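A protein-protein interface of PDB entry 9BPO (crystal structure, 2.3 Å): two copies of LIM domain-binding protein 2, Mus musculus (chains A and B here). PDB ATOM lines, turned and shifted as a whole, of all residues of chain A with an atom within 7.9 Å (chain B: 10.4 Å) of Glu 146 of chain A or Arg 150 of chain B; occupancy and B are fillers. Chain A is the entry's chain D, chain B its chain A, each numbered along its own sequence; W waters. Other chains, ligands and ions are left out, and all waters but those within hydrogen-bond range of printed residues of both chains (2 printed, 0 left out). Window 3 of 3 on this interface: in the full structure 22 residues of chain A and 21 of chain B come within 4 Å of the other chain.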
ATOM      1  N   THR A 106      14.912  28.551   5.458  1.00  0.00           N
ATOM      2  CA  THR A 106      14.915  30.012   5.393  1.00  0.00           C
ATOM      3  C   THR A 106      13.485  30.519   5.326  1.00  0.00           C
ATOM      4  O   THR A 106      12.672  29.968   4.581  1.00  0.00           O
ATOM      5  CB  THR A 106      15.701  30.552   4.190  1.00  0.00           C
ATOM      6  OG1 THR A 106      15.503  29.710   3.057  1.00  0.00           O
ATOM      7  CG2 THR A 106      17.163  30.576   4.520  1.00  0.00           C
ATOM      8  N   HIS A 108      11.018  33.658   4.408  1.00  0.00           N
ATOM      9  CA  HIS A 108      10.911  34.890   3.641  1.00  0.00           C
ATOM     10  C   HIS A 108       9.772  35.736   4.187  1.00  0.00           C
ATOM     11  O   HIS A 108       8.885  35.239   4.895  1.00  0.00           O
ATOM     12  CB  HIS A 108      10.670  34.598   2.160  1.00  0.00           C
ATOM     13  CG  HIS A 108      11.906  34.238   1.398  1.00  0.00           C
ATOM     14  ND1 HIS A 108      12.389  32.948   1.326  1.00  0.00           N
ATOM     15  CD2 HIS A 108      12.769  35.001   0.684  1.00  0.00           C
ATOM     16  CE1 HIS A 108      13.495  32.930   0.602  1.00  0.00           C
ATOM     17  NE2 HIS A 108      13.742  34.162   0.192  1.00  0.00           N
ATOM     18  N   MET A 112       5.151  36.671  -0.441  1.00  0.00           N
ATOM     19  CA  MET A 112       4.805  35.257  -0.412  1.00  0.00           C
ATOM     20  C   MET A 112       4.935  34.634   0.959  1.00  0.00           C
ATOM     21  O   MET A 112       4.253  33.636   1.239  1.00  0.00           O
ATOM     22  CB  MET A 112       5.699  34.479  -1.374  1.00  0.00           C
ATOM     23  CG  MET A 112       5.629  35.005  -2.778  1.00  0.00           C
ATOM     24  SD  MET A 112       4.165  34.548  -3.755  1.00  0.00           S
ATOM     25  CE  MET A 112       3.475  33.098  -2.940  1.00  0.00           C
ATOM     26  N   THR A 114       7.318  32.840   1.938  1.00  0.00           N
ATOM     27  CA  THR A 114       7.663  31.454   1.677  1.00  0.00           C
ATOM     28  C   THR A 114       8.564  30.901   2.775  1.00  0.00           C
ATOM     29  O   THR A 114       9.330  31.630   3.416  1.00  0.00           O
ATOM     30  CB  THR A 114       8.357  31.337   0.333  1.00  0.00           C
ATOM     31  OG1 THR A 114       7.666  32.170  -0.592  1.00  0.00           O
ATOM     32  CG2 THR A 114       8.356  29.883  -0.184  1.00  0.00           C
ATOM     33  N   LYS A 115       8.442  29.604   3.020  1.00  0.00           N
ATOM     34  CA  LYS A 115       9.447  28.857   3.782  1.00  0.00           C
ATOM     35  C   LYS A 115      10.168  27.925   2.829  1.00  0.00           C
ATOM     36  O   LYS A 115       9.540  27.036   2.238  1.00  0.00           O
ATOM     37  CB  LYS A 115       8.832  28.054   4.908  1.00  0.00           C
ATOM     38  CG  LYS A 115       9.831  27.619   5.919  1.00  0.00           C
ATOM     39  CD  LYS A 115       9.124  26.866   6.994  1.00  0.00           C
ATOM     40  CE  LYS A 115       8.763  27.804   8.113  1.00  0.00           C
ATOM     41  NZ  LYS A 115       8.070  27.055   9.210  1.00  0.00           N
ATOM     42  N   VAL A 116      11.470  28.131   2.678  1.00  0.00           N
ATOM     43  CA  VAL A 116      12.299  27.376   1.740  1.00  0.00           C
ATOM     44  C   VAL A 116      13.105  26.330   2.505  1.00  0.00           C
ATOM     45  O   VAL A 116      13.838  26.669   3.443  1.00  0.00           O
ATOM     46  CB  VAL A 116      13.237  28.320   0.972  1.00  0.00           C
ATOM     47  CG1 VAL A 116      14.252  27.514   0.170  1.00  0.00           C
ATOM     48  CG2 VAL A 116      12.448  29.257   0.101  1.00  0.00           C
ATOM     49  N   CYS A 117      13.007  25.064   2.096  1.00  0.00           N
ATOM     50  CA  CYS A 117      13.789  23.986   2.700  1.00  0.00           C
ATOM     51  C   CYS A 117      14.718  23.412   1.634  1.00  0.00           C
ATOM     52  O   CYS A 117      14.258  22.813   0.655  1.00  0.00           O
ATOM     53  CB  CYS A 117      12.900  22.884   3.283  1.00  0.00           C
ATOM     54  SG  CYS A 117      11.724  23.403   4.593  1.00  0.00           S
ATOM     55  N   THR A 118      16.018  23.563   1.843  1.00  0.00           N
ATOM     56  CA  THR A 118      17.039  22.956   0.990  1.00  0.00           C
ATOM     57  C   THR A 118      17.694  21.815   1.762  1.00  0.00           C
ATOM     58  O   THR A 118      18.188  22.015   2.879  1.00  0.00           O
ATOM     59  CB  THR A 118      18.056  24.009   0.549  1.00  0.00           C
ATOM     60  OG1 THR A 118      17.344  25.130   0.001  1.00  0.00           O
ATOM     61  CG2 THR A 118      19.003  23.464  -0.523  1.00  0.00           C
ATOM     62  N   TYR A 144      14.790  20.247  -2.717  1.00  0.00           N
ATOM     63  CA  TYR A 144      14.508  21.671  -2.613  1.00  0.00           C
ATOM     64  C   TYR A 144      13.006  21.889  -2.635  1.00  0.00           C
ATOM     65  O   TYR A 144      12.322  21.349  -3.506  1.00  0.00           O
ATOM     66  CB  TYR A 144      15.155  22.439  -3.761  1.00  0.00           C
ATOM     67  CG  TYR A 144      14.915  23.919  -3.703  1.00  0.00           C
ATOM     68  CD1 TYR A 144      15.662  24.719  -2.844  1.00  0.00           C
ATOM     69  CD2 TYR A 144      13.946  24.526  -4.511  1.00  0.00           C
ATOM     70  CE1 TYR A 144      15.462  26.076  -2.776  1.00  0.00           C
ATOM     71  CE2 TYR A 144      13.723  25.908  -4.456  1.00  0.00           C
ATOM     72  CZ  TYR A 144      14.486  26.662  -3.568  1.00  0.00           C
ATOM     73  OH  TYR A 144      14.314  28.007  -3.474  1.00  0.00           O
ATOM     74  N   ARG A 145      12.495  22.670  -1.691  1.00  0.00           N
ATOM     75  CA  ARG A 145      11.060  22.904  -1.621  1.00  0.00           C
ATOM     76  C   ARG A 145      10.810  24.350  -1.226  1.00  0.00           C
ATOM     77  O   ARG A 145      11.470  24.877  -0.325  1.00  0.00           O
ATOM     78  CB  ARG A 145      10.374  21.981  -0.605  1.00  0.00           C
ATOM     79  CG  ARG A 145      10.060  20.563  -1.068  1.00  0.00           C
ATOM     80  CD  ARG A 145       9.607  19.648   0.109  1.00  0.00           C
ATOM     81  NE  ARG A 145      10.374  19.889   1.333  1.00  0.00           N
ATOM     82  CZ  ARG A 145       9.917  19.765   2.578  1.00  0.00           C
ATOM     83  NH1 ARG A 145       8.644  19.493   2.833  1.00  0.00           N
ATOM     84  NH2 ARG A 145      10.771  19.887   3.599  1.00  0.00           N
ATOM     85  N   GLU A 146       9.868  24.989  -1.904  1.00  0.00           N
ATOM     86  CA  GLU A 146       9.399  26.314  -1.530  1.00  0.00           C
ATOM     87  C   GLU A 146       7.970  26.169  -1.035  1.00  0.00           C
ATOM     88  O   GLU A 146       7.058  25.908  -1.832  1.00  0.00           O
ATOM     89  CB  GLU A 146       9.485  27.270  -2.707  1.00  0.00           C
ATOM     90  CG  GLU A 146      10.908  27.702  -2.967  1.00  0.00           C
ATOM     91  CD  GLU A 146      11.032  28.583  -4.190  1.00  0.00           C
ATOM     92  OE1 GLU A 146       9.974  28.974  -4.744  1.00  0.00           O
ATOM     93  OE2 GLU A 146      12.184  28.888  -4.586  1.00  0.00           O
ATOM     94  N   LEU A 147       7.778  26.309   0.277  1.00  0.00           N
ATOM     95  CA  LEU A 147       6.476  26.102   0.897  1.00  0.00           C
ATOM     96  C   LEU A 147       5.770  27.449   1.104  1.00  0.00           C
ATOM     97  O   LEU A 147       6.346  28.385   1.673  1.00  0.00           O
ATOM     98  CB  LEU A 147       6.629  25.340   2.217  1.00  0.00           C
ATOM     99  CG  LEU A 147       7.432  24.036   2.078  1.00  0.00           C
ATOM    100  CD1 LEU A 147       8.510  23.956   3.154  1.00  0.00           C
ATOM    101  CD2 LEU A 147       6.532  22.830   2.167  1.00  0.00           C
ATOM    102  N   VAL A 148       4.532  27.531   0.638  1.00  0.00           N
ATOM    103  CA  VAL A 148       3.706  28.735   0.692  1.00  0.00           C
ATOM    104  C   VAL A 148       2.611  28.512   1.726  1.00  0.00           C
ATOM    105  O   VAL A 148       1.954  27.462   1.696  1.00  0.00           O
ATOM    106  CB  VAL A 148       3.073  29.052  -0.683  1.00  0.00           C
ATOM    107  CG1 VAL A 148       2.346  30.351  -0.642  1.00  0.00           C
ATOM    108  CG2 VAL A 148       4.120  29.075  -1.775  1.00  0.00           C
ATOM    109  N   PRO A 149       2.357  29.462   2.621  1.00  0.00           N
ATOM    110  CA  PRO A 149       1.205  29.330   3.521  1.00  0.00           C
ATOM    111  C   PRO A 149      -0.096  29.288   2.732  1.00  0.00           C
ATOM    112  O   PRO A 149      -0.329  30.096   1.815  1.00  0.00           O
ATOM    113  CB  PRO A 149       1.283  30.590   4.390  1.00  0.00           C
ATOM    114  CG  PRO A 149       1.984  31.599   3.502  1.00  0.00           C
ATOM    115  CD  PRO A 149       2.990  30.786   2.713  1.00  0.00           C
ATOM    116  N   GLN B 107       5.981  17.917  10.169  1.00  0.00           N
ATOM    117  CA  GLN B 107       6.018  17.647   8.732  1.00  0.00           C
ATOM    118  C   GLN B 107       5.057  16.513   8.392  1.00  0.00           C
ATOM    119  O   GLN B 107       5.186  15.404   8.925  1.00  0.00           O
ATOM    120  CB  GLN B 107       7.428  17.302   8.266  1.00  0.00           C
ATOM    121  CG  GLN B 107       7.461  16.779   6.837  1.00  0.00           C
ATOM    122  CD  GLN B 107       7.153  17.859   5.825  1.00  0.00           C
ATOM    123  OE1 GLN B 107       7.925  18.802   5.670  1.00  0.00           O
ATOM    124  NE2 GLN B 107       6.033  17.727   5.123  1.00  0.00           N
ATOM    125  N   MET B 112      -0.485  15.813   0.742  1.00  0.00           N
ATOM    126  CA  MET B 112      -0.187  17.250   0.710  1.00  0.00           C
ATOM    127  C   MET B 112       1.256  17.591   1.050  1.00  0.00           C
ATOM    128  O   MET B 112       1.753  18.643   0.616  1.00  0.00           O
ATOM    129  CB  MET B 112      -1.075  17.994   1.720  1.00  0.00           C
ATOM    130  CG  MET B 112      -2.544  18.095   1.378  1.00  0.00           C
ATOM    131  SD  MET B 112      -2.796  18.522  -0.340  1.00  0.00           S
ATOM    132  CE  MET B 112      -2.751  20.300  -0.180  1.00  0.00           C
ATOM    133  N   PHE B 113       1.914  16.749   1.864  1.00  0.00           N
ATOM    134  CA  PHE B 113       3.267  17.010   2.367  1.00  0.00           C
ATOM    135  C   PHE B 113       3.339  18.386   3.024  1.00  0.00           C
ATOM    136  O   PHE B 113       4.290  19.142   2.848  1.00  0.00           O
ATOM    137  CB  PHE B 113       4.311  16.848   1.253  1.00  0.00           C
ATOM    138  CG  PHE B 113       4.071  15.629   0.389  1.00  0.00           C
ATOM    139  CD1 PHE B 113       4.521  14.383   0.788  1.00  0.00           C
ATOM    140  CD2 PHE B 113       3.365  15.728  -0.791  1.00  0.00           C
ATOM    141  CE1 PHE B 113       4.286  13.252   0.004  1.00  0.00           C
ATOM    142  CE2 PHE B 113       3.122  14.601  -1.590  1.00  0.00           C
ATOM    143  CZ  PHE B 113       3.577  13.373  -1.191  1.00  0.00           C
ATOM    144  N   THR B 114       2.301  18.712   3.782  1.00  0.00           N
ATOM    145  CA  THR B 114       2.214  20.003   4.454  1.00  0.00           C
ATOM    146  C   THR B 114       3.238  20.132   5.579  1.00  0.00           C
ATOM    147  O   THR B 114       3.485  19.184   6.320  1.00  0.00           O
ATOM    148  CB  THR B 114       0.813  20.175   5.021  1.00  0.00           C
ATOM    149  OG1 THR B 114      -0.115  19.685   4.052  1.00  0.00           O
ATOM    150  CG2 THR B 114       0.507  21.637   5.328  1.00  0.00           C
ATOM    151  N   LYS B 115       3.849  21.304   5.689  1.00  0.00           N
ATOM    152  CA  LYS B 115       4.608  21.684   6.871  1.00  0.00           C
ATOM    153  C   LYS B 115       3.748  22.602   7.737  1.00  0.00           C
ATOM    154  O   LYS B 115       3.390  23.709   7.312  1.00  0.00           O
ATOM    155  CB  LYS B 115       5.922  22.372   6.497  1.00  0.00           C
ATOM    156  CG  LYS B 115       6.794  22.641   7.733  1.00  0.00           C
ATOM    157  CD  LYS B 115       8.170  23.114   7.365  1.00  0.00           C
ATOM    158  CE  LYS B 115       9.038  21.966   6.863  1.00  0.00           C
ATOM    159  NZ  LYS B 115      10.374  22.481   6.395  1.00  0.00           N
ATOM    160  N   GLU B 146      -0.201  26.528   7.606  1.00  0.00           N
ATOM    161  CA  GLU B 146      -0.051  25.246   6.921  1.00  0.00           C
ATOM    162  C   GLU B 146       0.603  25.544   5.583  1.00  0.00           C
ATOM    163  O   GLU B 146      -0.031  26.124   4.687  1.00  0.00           O
ATOM    164  CB  GLU B 146      -1.383  24.526   6.735  1.00  0.00           C
ATOM    165  CG  GLU B 146      -1.961  24.018   8.032  1.00  0.00           C
ATOM    166  CD  GLU B 146      -3.272  23.283   7.834  1.00  0.00           C
ATOM    167  OE1 GLU B 146      -3.651  23.054   6.655  1.00  0.00           O
ATOM    168  OE2 GLU B 146      -3.910  22.917   8.858  1.00  0.00           O
ATOM    169  N   LEU B 147       1.878  25.210   5.468  1.00  0.00           N
ATOM    170  CA  LEU B 147       2.653  25.570   4.296  1.00  0.00           C
ATOM    171  C   LEU B 147       2.668  24.385   3.338  1.00  0.00           C
ATOM    172  O   LEU B 147       2.900  23.249   3.758  1.00  0.00           O
ATOM    173  CB  LEU B 147       4.067  25.999   4.690  1.00  0.00           C
ATOM    174  CG  LEU B 147       4.103  27.134   5.720  1.00  0.00           C
ATOM    175  CD1 LEU B 147       4.854  26.662   6.961  1.00  0.00           C
ATOM    176  CD2 LEU B 147       4.764  28.376   5.122  1.00  0.00           C
ATOM    177  N   VAL B 148       2.401  24.649   2.063  1.00  0.00           N
ATOM    178  CA  VAL B 148       2.257  23.610   1.052  1.00  0.00           C
ATOM    179  C   VAL B 148       3.396  23.780   0.054  1.00  0.00           C
ATOM    180  O   VAL B 148       3.706  24.908  -0.323  1.00  0.00           O
ATOM    181  CB  VAL B 148       0.891  23.668   0.344  1.00  0.00           C
ATOM    182  CG1 VAL B 148       0.677  22.489  -0.578  1.00  0.00           C
ATOM    183  CG2 VAL B 148      -0.246  23.721   1.408  1.00  0.00           C
ATOM    184  N   PRO B 149       4.099  22.725  -0.330  1.00  0.00           N
ATOM    185  CA  PRO B 149       5.132  22.906  -1.351  1.00  0.00           C
ATOM    186  C   PRO B 149       4.465  23.344  -2.644  1.00  0.00           C
ATOM    187  O   PRO B 149       3.479  22.750  -3.083  1.00  0.00           O
ATOM    188  CB  PRO B 149       5.778  21.521  -1.472  1.00  0.00           C
ATOM    189  CG  PRO B 149       4.762  20.561  -0.930  1.00  0.00           C
ATOM    190  CD  PRO B 149       3.960  21.323   0.102  1.00  0.00           C
ATOM    191  N   ARG B 150       4.988  24.405  -3.241  1.00  0.00           N
ATOM    192  CA  ARG B 150       4.447  24.785  -4.533  1.00  0.00           C
ATOM    193  C   ARG B 150       5.082  23.939  -5.646  1.00  0.00           C
ATOM    194  O   ARG B 150       6.126  23.309  -5.472  1.00  0.00           O
ATOM    195  CB  ARG B 150       4.660  26.281  -4.785  1.00  0.00           C
ATOM    196  CG  ARG B 150       6.056  26.629  -5.329  1.00  0.00           C
ATOM    197  CD  ARG B 150       6.304  28.111  -5.135  1.00  0.00           C
ATOM    198  NE  ARG B 150       7.584  28.558  -5.670  1.00  0.00           N
ATOM    199  CZ  ARG B 150       7.861  28.692  -6.960  1.00  0.00           C
ATOM    200  NH1 ARG B 150       7.017  28.286  -7.896  1.00  0.00           N
ATOM    201  NH2 ARG B 150       9.011  29.258  -7.320  1.00  0.00           N
ATOM    202  N   SER B 151       4.406  23.901  -6.795  1.00  0.00           N
ATOM    203  CA  SER B 151       4.932  23.219  -7.973  1.00  0.00           C
ATOM    204  C   SER B 151       5.879  24.177  -8.679  1.00  0.00           C
ATOM    205  O   SER B 151       5.450  25.183  -9.239  1.00  0.00           O
ATOM    206  CB  SER B 151       3.808  22.773  -8.898  1.00  0.00           C
ATOM    207  OG  SER B 151       4.361  22.196 -10.058  1.00  0.00           O
ATOM    208  N   ILE B 152       7.171  23.853  -8.664  1.00  0.00           N
ATOM    209  CA  ILE B 152       8.198  24.824  -9.016  1.00  0.00           C
ATOM    210  C   ILE B 152       8.358  24.956 -10.519  1.00  0.00           C
ATOM    211  O   ILE B 152       8.646  26.053 -11.013  1.00  0.00           O
ATOM    212  CB  ILE B 152       9.519  24.427  -8.336  1.00  0.00           C
ATOM    213  CG1 ILE B 152       9.424  24.740  -6.825  1.00  0.00           C
ATOM    214  CG2 ILE B 152      10.686  25.117  -8.991  1.00  0.00           C
ATOM    215  CD1 ILE B 152      10.648  24.374  -6.051  1.00  0.00           C
ATOM    216  N   LEU B 153       8.166  23.870 -11.268  1.00  0.00           N
ATOM    217  CA  LEU B 153       8.367  23.855 -12.713  1.00  0.00           C
ATOM    218  C   LEU B 153       7.068  23.534 -13.448  1.00  0.00           C
ATOM    219  O   LEU B 153       6.246  22.725 -12.984  1.00  0.00           O
ATOM    220  CB  LEU B 153       9.439  22.843 -13.103  1.00  0.00           C
ATOM    221  CG  LEU B 153      10.841  23.188 -12.606  1.00  0.00           C
ATOM    222  CD1 LEU B 153      11.817  22.061 -12.907  1.00  0.00           C
ATOM    223  CD2 LEU B 153      11.319  24.517 -13.176  1.00  0.00           C
ATOM    224  N   ALA B 154       6.895  24.170 -14.607  1.00  0.00           N
ATOM    225  CA  ALA B 154       5.675  23.979 -15.385  1.00  0.00           C
ATOM    226  C   ALA B 154       5.517  22.528 -15.817  1.00  0.00           C
ATOM    227  O   ALA B 154       4.430  21.956 -15.687  1.00  0.00           O
ATOM    228  CB  ALA B 154       5.677  24.916 -16.591  1.00  0.00           C
ATOM    229  N   HIS B 156       6.076  19.956 -14.385  1.00  0.00           N
ATOM    230  CA  HIS B 156       5.581  19.064 -13.337  1.00  0.00           C
ATOM    231  C   HIS B 156       4.123  18.689 -13.577  1.00  0.00           C
ATOM    232  O   HIS B 156       3.723  17.541 -13.341  1.00  0.00           O
ATOM    233  CB  HIS B 156       5.737  19.704 -11.953  1.00  0.00           C
ATOM    234  CG  HIS B 156       7.148  19.733 -11.450  1.00  0.00           C
ATOM    235  ND1 HIS B 156       8.159  18.979 -12.015  1.00  0.00           N
ATOM    236  CD2 HIS B 156       7.723  20.447 -10.448  1.00  0.00           C
ATOM    237  CE1 HIS B 156       9.291  19.214 -11.370  1.00  0.00           C
ATOM    238  NE2 HIS B 156       9.053  20.102 -10.418  1.00  0.00           N
ATOM    239  N   ALA B 157       3.311  19.628 -14.080  1.00  0.00           N
ATOM    240  CA  ALA B 157       1.913  19.285 -14.341  1.00  0.00           C
ATOM    241  C   ALA B 157       1.744  18.258 -15.464  1.00  0.00           C
ATOM    242  O   ALA B 157       0.645  17.709 -15.618  1.00  0.00           O
ATOM    243  CB  ALA B 157       1.113  20.554 -14.648  1.00  0.00           C
HETATM  244  O   HOH W   1       7.994  23.462  -3.520  1.00  0.00           O
HETATM  245  O   HOH W   2       6.608  19.302   1.280  1.00  0.00           O
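Among the printed residues, merely in contact across the chains: Lys 115 of chain A with Lys 115 of chain B (3.9 Å), Lys 115 of chain A with Leu 147 of chain B (3.9 Å), Tyr 144 of chain A with Ile 152 of chain B (3.6 Å), Arg 145 of chain A with Lys 115 of chain B (3.8 Å), Glu 146 of chain A with Val 148 of chain B (3.8 Å), Glu 146 of chain A with Pro 149 of chain B (3.6 Å), Leu 147 of chain A with Leu 147 of chain B (3.6 Å), Leu 147 of chain A with Val 148 of chain B (3.3 Å), Leu 147 of chain A with Pro 149 of chain B (3.5 Å), Val 148 of chain A with Glu 146 of chain B (3.8 Å), Val 148 of chain A with Leu 147 of chain B (3.3 Å), Pro 149 of chain A with Glu 146 of chain B (3.6 Å) and Pro 149 of chain A with Leu 147 of chain B (3.6 Å).
Thr 118 of chain A touches none of the printed residues of chain B.
Glu 146 of chain A touches just these residues of chain B: Val 148, Pro 149 and Arg 150.
Of the printed residues of chain B, Pro 149 of chain A touches Glu 146 (3.6 Å) and Leu 147 (3.6 Å).
Of the printed residues of chain A, Lys 115 of chain B touches Lys 115 (3.9 Å), Cys 117 (2.4 Å) and Arg 145 (3.8 Å).
Printed residues of chain A within 4 Å of Pro 149 of chain B: Glu 146 (3.6 Å) and Leu 147 (3.5 Å).
Of chain A, only Glu 146 (2.6 Å) comes within 4 Å of Arg 150 of chain B.
Ala 154 of chain B touches none of the printed residues of chain A.
The nearest residue of chain B that does not touch Glu 146 of chain A is Ile 152 of chain B (4.3 Å).
The nearest residue of chain A that does not touch Arg 150 of chain B is Val 148 of chain A (4.1 Å).
The nearest printed residue of chain A that does not touch Leu 147 of chain B is Thr 114 of chain A (5.1 Å).
Water W2 bridges the guanidinium group of Arg 145 of chain A and the backbone carbonyl oxygen of Phe 113 of chain B.
Water W1 bridges O of Arg 150 of chain B and N of Glu 146 of chain A.
Glu 146 of chain A touches Val 148 of chain B, and with the chains exchanged Val 148 of chain A touches Glu 146 of chain B.
Leu 147 of chain B touches its own counterpart, Leu 147 of chain A.
Leu 147 of chain A touches Val 148 of chain B, and with the chains exchanged Val 148 of chain A touches Leu 147 of chain B.
Leu 147 of chain A touches Pro 149 of chain B, and with the chains exchanged Pro 149 of chain A touches Leu 147 of chain B.
7 positions are printed for both chains.
Of the 17 pairs that touch across the chains among the printed residues, 11 have their exchanged pair printed and touching as well.
Hydrophobic or aromatic side chains of chain A within 4 Å of the printed part of chain B: Tyr 144, Leu 147 and Pro 149.
Along chain A the printed residues that touch a printed residue of chain B span positions 115 to 149.
N of Leu 147 of chain B is in hydrogen-bond range of O of Lys 115 of chain B (2.8 Å).
O of Lys 115 of chain A sits at hydrogen-bond distance from N of Leu 147 of chain A (2.7 Å).
O of Thr 114 of chain B sits at hydrogen-bond distance from NE2 of Gln 107 of chain B, 3.2 Å away.
The side-chain carboxylate (OE2) of Glu 146 of chain A lies within hydrogen-bond range of the side-chain hydroxyl (OH) of Tyr 144 of chain A (2.6 Å).
The backbone NH of Cys 117 of chain A sits at hydrogen-bond distance from the backbone carbonyl oxygen of Arg 145 of chain A (2.9 Å).
The side-chain amide nitrogen of Gln 107 of chain B sits at hydrogen-bond distance from the backbone carbonyl oxygen of Phe 113 of chain B (3.2 Å).
The side-chain amino group (NZ) of Lys 115 of chain B is in hydrogen-bond range of the side-chain sulfur (SG) of Cys 117 of chain A, at 2.4 Å.
The guanidinium group (NH1) of Arg 145 of chain A sits at hydrogen-bond distance from the side-chain amide oxygen (OE1) of Gln 107 of chain B.
The backbone NH (N) of Val 148 of chain B is in hydrogen-bond range of the backbone carbonyl oxygen (O) of Val 148 of chain A (2.9 Å).
OE1 of Glu 146 of chain A is in salt-bridge range of NE of Arg 150 of chain B (2.6 Å).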
